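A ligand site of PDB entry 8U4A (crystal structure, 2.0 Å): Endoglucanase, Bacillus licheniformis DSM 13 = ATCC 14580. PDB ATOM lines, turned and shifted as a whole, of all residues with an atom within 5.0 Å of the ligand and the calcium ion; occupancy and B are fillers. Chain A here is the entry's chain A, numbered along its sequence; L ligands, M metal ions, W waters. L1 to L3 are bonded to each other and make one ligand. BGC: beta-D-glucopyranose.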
ATOM      1  N   ASP A 153      -2.781 -21.093  27.134  1.00  0.00           N
ATOM      2  CA  ASP A 153      -3.322 -20.297  28.237  1.00  0.00           C
ATOM      3  C   ASP A 153      -3.847 -21.195  29.345  1.00  0.00           C
ATOM      4  O   ASP A 153      -3.469 -21.052  30.513  1.00  0.00           O
ATOM      5  CB  ASP A 153      -4.407 -19.311  27.726  1.00  0.00           C
ATOM      6  CG  ASP A 153      -5.209 -19.856  26.528  1.00  0.00           C
ATOM      7  OD1 ASP A 153      -5.337 -21.087  26.351  1.00  0.00           O
ATOM      8  OD2 ASP A 153      -5.720 -19.022  25.723  1.00  0.00           O
ATOM      9  N   SER A 211     -10.648 -16.682  25.372  1.00  0.00           N
ATOM     10  CA  SER A 211      -9.263 -16.232  25.581  1.00  0.00           C
ATOM     11  C   SER A 211      -9.101 -14.881  24.872  1.00  0.00           C
ATOM     12  O   SER A 211      -8.579 -14.776  23.766  1.00  0.00           O
ATOM     13  CB  SER A 211      -8.245 -17.242  25.084  1.00  0.00           C
ATOM     14  OG  SER A 211      -6.902 -16.768  25.366  1.00  0.00           O
ATOM     15  N   TRP A 212      -9.600 -13.831  25.526  1.00  0.00           N
ATOM     16  CA  TRP A 212      -9.537 -12.500  24.912  1.00  0.00           C
ATOM     17  C   TRP A 212      -8.101 -12.093  24.647  1.00  0.00           C
ATOM     18  O   TRP A 212      -7.760 -11.690  23.541  1.00  0.00           O
ATOM     19  CB  TRP A 212     -10.225 -11.475  25.794  1.00  0.00           C
ATOM     20  CG  TRP A 212     -11.683 -11.814  26.048  1.00  0.00           C
ATOM     21  CD1 TRP A 212     -12.200 -12.431  27.155  1.00  0.00           C
ATOM     22  CD2 TRP A 212     -12.782 -11.612  25.141  1.00  0.00           C
ATOM     23  NE1 TRP A 212     -13.572 -12.604  26.990  1.00  0.00           N
ATOM     24  CE2 TRP A 212     -13.951 -12.084  25.781  1.00  0.00           C
ATOM     25  CE3 TRP A 212     -12.893 -11.050  23.858  1.00  0.00           C
ATOM     26  CZ2 TRP A 212     -15.202 -12.032  25.194  1.00  0.00           C
ATOM     27  CZ3 TRP A 212     -14.148 -11.001  23.262  1.00  0.00           C
ATOM     28  CH2 TRP A 212     -15.284 -11.478  23.933  1.00  0.00           C
ATOM     29  N   SER A 213      -7.207 -12.258  25.640  1.00  0.00           N
ATOM     30  CA  SER A 213      -5.857 -11.745  25.598  1.00  0.00           C
ATOM     31  C   SER A 213      -4.877 -12.707  24.917  1.00  0.00           C
ATOM     32  O   SER A 213      -3.726 -12.308  24.642  1.00  0.00           O
ATOM     33  CB  SER A 213      -5.359 -11.472  27.013  1.00  0.00           C
ATOM     34  OG  SER A 213      -5.364 -12.678  27.779  1.00  0.00           O
ATOM     35  N   GLY A 214      -5.274 -13.943  24.651  1.00  0.00           N
ATOM     36  CA  GLY A 214      -4.287 -14.860  24.117  1.00  0.00           C
ATOM     37  C   GLY A 214      -3.507 -15.485  25.252  1.00  0.00           C
ATOM     38  O   GLY A 214      -3.878 -15.384  26.421  1.00  0.00           O
ATOM     39  N   TYR A 215      -2.403 -16.158  24.918  1.00  0.00           N
ATOM     40  CA  TYR A 215      -1.716 -17.005  25.891  1.00  0.00           C
ATOM     41  C   TYR A 215      -0.334 -16.491  26.257  1.00  0.00           C
ATOM     42  O   TYR A 215       0.337 -17.118  27.085  1.00  0.00           O
ATOM     43  CB  TYR A 215      -1.614 -18.452  25.356  1.00  0.00           C
ATOM     44  CG  TYR A 215      -0.998 -18.563  23.964  1.00  0.00           C
ATOM     45  CD1 TYR A 215       0.376 -18.388  23.773  1.00  0.00           C
ATOM     46  CD2 TYR A 215      -1.780 -18.824  22.851  1.00  0.00           C
ATOM     47  CE1 TYR A 215       0.956 -18.464  22.483  1.00  0.00           C
ATOM     48  CE2 TYR A 215      -1.198 -18.891  21.557  1.00  0.00           C
ATOM     49  CZ  TYR A 215       0.159 -18.723  21.389  1.00  0.00           C
ATOM     50  OH  TYR A 215       0.746 -18.832  20.130  1.00  0.00           O
ATOM     51  N   ASP A 217       0.559 -14.135  28.098  1.00  0.00           N
ATOM     52  CA  ASP A 217       0.683 -13.788  29.512  1.00  0.00           C
ATOM     53  C   ASP A 217       0.780 -15.055  30.373  1.00  0.00           C
ATOM     54  O   ASP A 217       1.555 -15.083  31.350  1.00  0.00           O
ATOM     55  CB  ASP A 217      -0.491 -12.898  29.955  1.00  0.00           C
ATOM     56  CG  ASP A 217      -1.866 -13.429  29.508  1.00  0.00           C
ATOM     57  OD1 ASP A 217      -2.084 -13.614  28.291  1.00  0.00           O
ATOM     58  OD2 ASP A 217      -2.753 -13.628  30.379  1.00  0.00           O
ATOM     59  N   GLU A 218      -0.002 -16.098  30.061  1.00  0.00           N
ATOM     60  CA  GLU A 218       0.075 -17.341  30.842  1.00  0.00           C
ATOM     61  C   GLU A 218       1.420 -18.035  30.645  1.00  0.00           C
ATOM     62  O   GLU A 218       1.916 -18.712  31.559  1.00  0.00           O
ATOM     63  CB  GLU A 218      -1.076 -18.296  30.439  1.00  0.00           C
ATOM     64  CG  GLU A 218      -2.448 -17.863  30.984  1.00  0.00           C
ATOM     65  CD  GLU A 218      -3.210 -16.832  30.119  1.00  0.00           C
ATOM     66  OE1 GLU A 218      -2.766 -16.491  28.989  1.00  0.00           O
ATOM     67  OE2 GLU A 218      -4.295 -16.389  30.555  1.00  0.00           O
ATOM     68  N   PRO A 253       0.172  -3.241  27.944  1.00  0.00           N
ATOM     69  CA  PRO A 253      -1.101  -2.705  28.450  1.00  0.00           C
ATOM     70  C   PRO A 253      -0.995  -2.331  29.935  1.00  0.00           C
ATOM     71  O   PRO A 253      -0.281  -2.972  30.709  1.00  0.00           O
ATOM     72  CB  PRO A 253      -2.079  -3.872  28.224  1.00  0.00           C
ATOM     73  CG  PRO A 253      -1.193  -5.090  28.398  1.00  0.00           C
ATOM     74  CD  PRO A 253       0.109  -4.696  27.713  1.00  0.00           C
ATOM     75  N   ARG A 255      -4.271  -0.459  31.227  1.00  0.00           N
ATOM     76  CA  ARG A 255      -5.614   0.017  31.589  1.00  0.00           C
ATOM     77  C   ARG A 255      -6.567  -1.094  32.052  1.00  0.00           C
ATOM     78  O   ARG A 255      -7.740  -0.791  32.333  1.00  0.00           O
ATOM     79  CB  ARG A 255      -6.255   0.733  30.410  1.00  0.00           C
ATOM     80  CG  ARG A 255      -5.563   2.044  30.033  1.00  0.00           C
ATOM     81  CD  ARG A 255      -6.142   2.575  28.715  1.00  0.00           C
ATOM     82  NE  ARG A 255      -5.492   3.808  28.292  1.00  0.00           N
ATOM     83  CZ  ARG A 255      -5.271   4.157  27.031  1.00  0.00           C
ATOM     84  NH1 ARG A 255      -5.577   3.348  26.032  1.00  0.00           N
ATOM     85  NH2 ARG A 255      -4.704   5.341  26.774  1.00  0.00           N
ATOM     86  N   TRP A 256      -6.122  -2.348  32.120  1.00  0.00           N
ATOM     87  CA  TRP A 256      -6.971  -3.399  32.720  1.00  0.00           C
ATOM     88  C   TRP A 256      -6.377  -3.762  34.093  1.00  0.00           C
ATOM     89  O   TRP A 256      -5.766  -2.895  34.732  1.00  0.00           O
ATOM     90  CB  TRP A 256      -7.075  -4.573  31.733  1.00  0.00           C
ATOM     91  CG  TRP A 256      -8.325  -5.332  31.838  1.00  0.00           C
ATOM     92  CD1 TRP A 256      -8.486  -6.623  32.360  1.00  0.00           C
ATOM     93  CD2 TRP A 256      -9.643  -4.880  31.485  1.00  0.00           C
ATOM     94  NE1 TRP A 256      -9.831  -6.971  32.345  1.00  0.00           N
ATOM     95  CE2 TRP A 256     -10.556  -5.915  31.843  1.00  0.00           C
ATOM     96  CE3 TRP A 256     -10.144  -3.700  30.940  1.00  0.00           C
ATOM     97  CZ2 TRP A 256     -11.939  -5.813  31.605  1.00  0.00           C
ATOM     98  CZ3 TRP A 256     -11.513  -3.589  30.727  1.00  0.00           C
ATOM     99  CH2 TRP A 256     -12.403  -4.654  31.058  1.00  0.00           C
ATOM    100  N   SER A 259      -6.742 -10.650  36.095  1.00  0.00           N
ATOM    101  CA  SER A 259      -8.060 -11.219  35.866  1.00  0.00           C
ATOM    102  C   SER A 259      -7.873 -12.651  35.387  1.00  0.00           C
ATOM    103  O   SER A 259      -6.759 -13.059  35.042  1.00  0.00           O
ATOM    104  CB  SER A 259      -8.856 -10.406  34.832  1.00  0.00           C
ATOM    105  OG  SER A 259      -8.138 -10.368  33.620  1.00  0.00           O
ATOM    106  N   TRP A 260      -8.986 -13.406  35.358  1.00  0.00           N
ATOM    107  CA  TRP A 260      -8.918 -14.800  34.917  1.00  0.00           C
ATOM    108  C   TRP A 260      -8.356 -14.916  33.509  1.00  0.00           C
ATOM    109  O   TRP A 260      -7.717 -15.924  33.168  1.00  0.00           O
ATOM    110  CB  TRP A 260     -10.295 -15.492  34.973  1.00  0.00           C
ATOM    111  CG  TRP A 260     -11.351 -14.805  34.132  1.00  0.00           C
ATOM    112  CD1 TRP A 260     -12.244 -13.879  34.541  1.00  0.00           C
ATOM    113  CD2 TRP A 260     -11.561 -14.981  32.719  1.00  0.00           C
ATOM    114  NE1 TRP A 260     -12.995 -13.419  33.458  1.00  0.00           N
ATOM    115  CE2 TRP A 260     -12.599 -14.106  32.337  1.00  0.00           C
ATOM    116  CE3 TRP A 260     -10.960 -15.795  31.732  1.00  0.00           C
ATOM    117  CZ2 TRP A 260     -13.098 -14.071  31.046  1.00  0.00           C
ATOM    118  CZ3 TRP A 260     -11.416 -15.706  30.459  1.00  0.00           C
ATOM    119  CH2 TRP A 260     -12.462 -14.856  30.113  1.00  0.00           C
ATOM    120  N   ASP A 261      -8.569 -13.896  32.661  1.00  0.00           N
ATOM    121  CA  ASP A 261      -8.104 -13.954  31.297  1.00  0.00           C
ATOM    122  C   ASP A 261      -6.741 -13.333  31.107  1.00  0.00           C
ATOM    123  O   ASP A 261      -6.026 -13.738  30.184  1.00  0.00           O
ATOM    124  CB  ASP A 261      -9.058 -13.223  30.339  1.00  0.00           C
ATOM    125  CG  ASP A 261      -8.594 -13.358  28.883  1.00  0.00           C
ATOM    126  OD1 ASP A 261      -8.704 -14.480  28.390  1.00  0.00           O
ATOM    127  OD2 ASP A 261      -8.008 -12.399  28.277  1.00  0.00           O
ATOM    128  N   ASP A 262      -6.367 -12.337  31.913  1.00  0.00           N
ATOM    129  CA  ASP A 262      -5.118 -11.610  31.667  1.00  0.00           C
ATOM    130  C   ASP A 262      -4.270 -11.615  32.927  1.00  0.00           C
ATOM    131  O   ASP A 262      -4.533 -10.880  33.888  1.00  0.00           O
ATOM    132  CB  ASP A 262      -5.384 -10.197  31.191  1.00  0.00           C
ATOM    133  CG  ASP A 262      -4.142  -9.562  30.552  1.00  0.00           C
ATOM    134  OD1 ASP A 262      -3.050 -10.021  30.957  1.00  0.00           O
ATOM    135  OD2 ASP A 262      -4.282  -8.648  29.688  1.00  0.00           O
ATOM    136  N   VAL A 263      -3.243 -12.463  32.951  1.00  0.00           N
ATOM    137  CA  VAL A 263      -2.353 -12.501  34.117  1.00  0.00           C
ATOM    138  C   VAL A 263      -1.082 -11.676  33.873  1.00  0.00           C
ATOM    139  O   VAL A 263      -0.117 -11.812  34.630  1.00  0.00           O
ATOM    140  CB  VAL A 263      -2.036 -13.955  34.532  1.00  0.00           C
ATOM    141  CG1 VAL A 263      -3.247 -14.581  35.210  1.00  0.00           C
ATOM    142  CG2 VAL A 263      -1.551 -14.833  33.321  1.00  0.00           C
ATOM    143  N   TYR A 265      -0.578  -8.768  34.595  1.00  0.00           N
ATOM    144  CA  TYR A 265      -0.394  -7.900  35.747  1.00  0.00           C
ATOM    145  C   TYR A 265       0.189  -8.668  36.927  1.00  0.00           C
ATOM    146  O   TYR A 265       0.953  -8.111  37.717  1.00  0.00           O
ATOM    147  CB  TYR A 265      -1.736  -7.243  36.084  1.00  0.00           C
ATOM    148  CG  TYR A 265      -2.315  -6.482  34.891  1.00  0.00           C
ATOM    149  CD1 TYR A 265      -1.921  -5.176  34.652  1.00  0.00           C
ATOM    150  CD2 TYR A 265      -3.208  -7.078  33.995  1.00  0.00           C
ATOM    151  CE1 TYR A 265      -2.395  -4.473  33.588  1.00  0.00           C
ATOM    152  CE2 TYR A 265      -3.700  -6.357  32.863  1.00  0.00           C
ATOM    153  CZ  TYR A 265      -3.276  -5.040  32.687  1.00  0.00           C
ATOM    154  OH  TYR A 265      -3.722  -4.252  31.627  1.00  0.00           O
ATOM    155  N   GLU A 315     -15.630  -1.870  34.658  1.00  0.00           N
ATOM    156  CA  GLU A 315     -16.698  -2.122  33.695  1.00  0.00           C
ATOM    157  C   GLU A 315     -17.906  -2.735  34.425  1.00  0.00           C
ATOM    158  O   GLU A 315     -17.843  -3.034  35.613  1.00  0.00           O
ATOM    159  CB  GLU A 315     -16.218  -3.022  32.553  1.00  0.00           C
ATOM    160  CG  GLU A 315     -15.806  -4.411  32.990  1.00  0.00           C
ATOM    161  CD  GLU A 315     -16.233  -5.519  31.965  1.00  0.00           C
ATOM    162  OE1 GLU A 315     -17.131  -5.265  31.158  1.00  0.00           O
ATOM    163  OE2 GLU A 315     -15.684  -6.652  31.985  1.00  0.00           O
ATOM    164  N   TYR A 322     -13.016  -6.690  39.924  1.00  0.00           N
ATOM    165  CA  TYR A 322     -11.902  -5.958  39.323  1.00  0.00           C
ATOM    166  C   TYR A 322     -11.192  -5.065  40.337  1.00  0.00           C
ATOM    167  O   TYR A 322      -9.955  -5.017  40.356  1.00  0.00           O
ATOM    168  CB  TYR A 322     -12.364  -5.122  38.137  1.00  0.00           C
ATOM    169  CG  TYR A 322     -12.656  -5.999  36.928  1.00  0.00           C
ATOM    170  CD1 TYR A 322     -11.687  -6.904  36.483  1.00  0.00           C
ATOM    171  CD2 TYR A 322     -13.895  -5.961  36.268  1.00  0.00           C
ATOM    172  CE1 TYR A 322     -11.928  -7.736  35.350  1.00  0.00           C
ATOM    173  CE2 TYR A 322     -14.164  -6.781  35.170  1.00  0.00           C
ATOM    174  CZ  TYR A 322     -13.186  -7.651  34.708  1.00  0.00           C
ATOM    175  OH  TYR A 322     -13.456  -8.446  33.638  1.00  0.00           O
HETATM  176  C2  BGC L   1     -14.415  -9.190  29.341  1.00  0.00           C
HETATM  177  C3  BGC L   1     -13.072  -9.119  28.622  1.00  0.00           C
HETATM  178  C4  BGC L   1     -11.914  -9.265  29.585  1.00  0.00           C
HETATM  179  C5  BGC L   1     -12.093 -10.511  30.458  1.00  0.00           C
HETATM  180  C6  BGC L   1     -11.027 -10.656  31.541  1.00  0.00           C
HETATM  181  C1  BGC L   1     -14.478 -10.449  30.227  1.00  0.00           C
HETATM  182  O1  BGC L   1     -15.643 -10.454  30.970  1.00  0.00           O
HETATM  183  O2  BGC L   1     -15.472  -9.246  28.390  1.00  0.00           O
HETATM  184  O3  BGC L   1     -12.953  -7.920  27.857  1.00  0.00           O
HETATM  185  O4  BGC L   1     -10.747  -9.452  28.797  1.00  0.00           O
HETATM  186  O5  BGC L   1     -13.369 -10.465  31.126  1.00  0.00           O
HETATM  187  O6  BGC L   1     -11.080  -9.573  32.465  1.00  0.00           O
HETATM  188  C2  BGC L   2      -8.453  -8.825  28.485  1.00  0.00           C
HETATM  189  C3  BGC L   2      -7.466  -7.680  28.548  1.00  0.00           C
HETATM  190  C4  BGC L   2      -7.975  -6.445  27.800  1.00  0.00           C
HETATM  191  C5  BGC L   2      -9.390  -6.115  28.295  1.00  0.00           C
HETATM  192  C6  BGC L   2     -10.072  -4.964  27.585  1.00  0.00           C
HETATM  193  C1  BGC L   2      -9.835  -8.348  28.926  1.00  0.00           C
HETATM  194  O2  BGC L   2      -7.990  -9.898  29.287  1.00  0.00           O
HETATM  195  O3  BGC L   2      -6.239  -8.146  27.997  1.00  0.00           O
HETATM  196  O4  BGC L   2      -7.144  -5.360  28.131  1.00  0.00           O
HETATM  197  O5  BGC L   2     -10.230  -7.266  28.108  1.00  0.00           O
HETATM  198  O6  BGC L   2     -10.207  -5.189  26.184  1.00  0.00           O
HETATM  199  C2  BGC L   3      -6.383  -3.143  27.643  1.00  0.00           C
HETATM  200  C3  BGC L   3      -6.076  -2.182  26.501  1.00  0.00           C
HETATM  201  C4  BGC L   3      -5.093  -2.814  25.509  1.00  0.00           C
HETATM  202  C5  BGC L   3      -5.537  -4.238  25.129  1.00  0.00           C
HETATM  203  C6  BGC L   3      -4.473  -5.027  24.406  1.00  0.00           C
HETATM  204  C1  BGC L   3      -6.861  -4.463  27.058  1.00  0.00           C
HETATM  205  O2  BGC L   3      -7.429  -2.624  28.481  1.00  0.00           O
HETATM  206  O3  BGC L   3      -5.585  -0.941  26.999  1.00  0.00           O
HETATM  207  O4  BGC L   3      -5.074  -2.056  24.305  1.00  0.00           O
HETATM  208  O5  BGC L   3      -5.849  -5.011  26.283  1.00  0.00           O
HETATM  209  O6  BGC L   3      -5.115  -6.050  23.657  1.00  0.00           O
HETATM  210 CA    CA M   1      -4.318 -14.680  28.693  1.00  0.00          CA
HETATM  211  O   HOH W   1      -6.403 -15.674  27.904  1.00  0.00           O
HETATM  212  O   HOH W   2      -3.419  -0.218  28.247  1.00  0.00           O
HETATM  213  O   HOH W   3      -4.591  -5.951  29.722  1.00  0.00           O
HETATM  214  O   HOH W   4      -7.415   1.026  25.961  1.00  0.00           O
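The side-chain carboxylate (OD2) of Asp 217 lies close to the backbone NH (N) of Val 263 (2.9 Å).
The side-chain hydroxyl of Tyr 265 lies within hydrogen-bond range of the backbone NH of Trp 256, at 3.1 Å.
The side-chain hydroxyl (OG) of Ser 259 sits at hydrogen-bond distance from the backbone NH (N) of Asp 262.
The side-chain carboxylate (OE2) of Glu 315 lies within hydrogen-bond range of the side-chain hydroxyl (OH) of Tyr 322.
The side-chain hydroxyl of Ser 211 is in hydrogen-bond range of the backbone NH of Gly 214, 3.3 Å away.
N of Trp 212 sits at hydrogen-bond distance from OD1 of Asp 261, 3.1 Å away.
The side-chain carboxylate (OE1) of Glu 218 is bound to the calcium ion, 2.4 Å away.
O of Gly 214 binds the calcium ion (2.4 Å).
OG of Ser 213 binds the calcium ion, at 2.4 Å.
The calcium ion is bound by water W1 (2.4 Å).
The calcium ion is bound by O of Asp 261 (2.5 Å).
The side-chain carboxylate (OD1) of Asp 217 binds the calcium ion (2.5 Å).
The calcium ion is bound by the side-chain carboxylate (OE2) of Glu 218 (2.5 Å).
OD2 of Asp 217 binds the calcium ion, 2.5 Å away.
OD2 of Asp 262 is in hydrogen-bond range of O3 of BGC L2 (2.6 Å).
OG of Ser 259 lies within hydrogen-bond range of O6 of BGC L1 (3.3 Å).
The side-chain carboxylate (OD2) of Asp 261 lies within hydrogen-bond range of an oxygen (O2) of BGC L2 (2.7 Å).
An oxygen (O6) of BGC L1 is in hydrogen-bond range of the side-chain hydroxyl (OH) of Tyr 322, at 2.9 Å.
The indole nitrogen (NE1) of Trp 256 lies within hydrogen-bond range of an oxygen (O6) of BGC L1, at 2.9 Å.
Within 4 Å of the calcium ion: Ser 213, Gly 214, Asp 217, Glu 218 and Asp 261.
The nearest printed residue that does not touch the calcium ion is Asp 262 (4.3 Å).
Trp 212 touches the ligand.
Arg 255 touches the ligand.
CZ2 of Trp 260 touches O5 of BGC L1, at 3.6 Å.
OE2 of Glu 315 touches C2 of BGC L1, at 3.9 Å.
Water W1 lies within hydrogen-bond range of OD1 of Asp 261 and OG of Ser 211.
Water W2 lies within hydrogen-bond range of an oxygen (O3) of BGC L3 and the backbone NH of Arg 255.
Water W4 lies within hydrogen-bond range of an oxygen (O3) of BGC L3 (2.9 Å) and the guanidinium group of Arg 255 (3.0 Å).
Water W3 lies within hydrogen-bond range of the side-chain hydroxyl (OH) of Tyr 265, the side-chain carboxylate (OD2) of Asp 262 and an oxygen (O4) of BGC L2.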
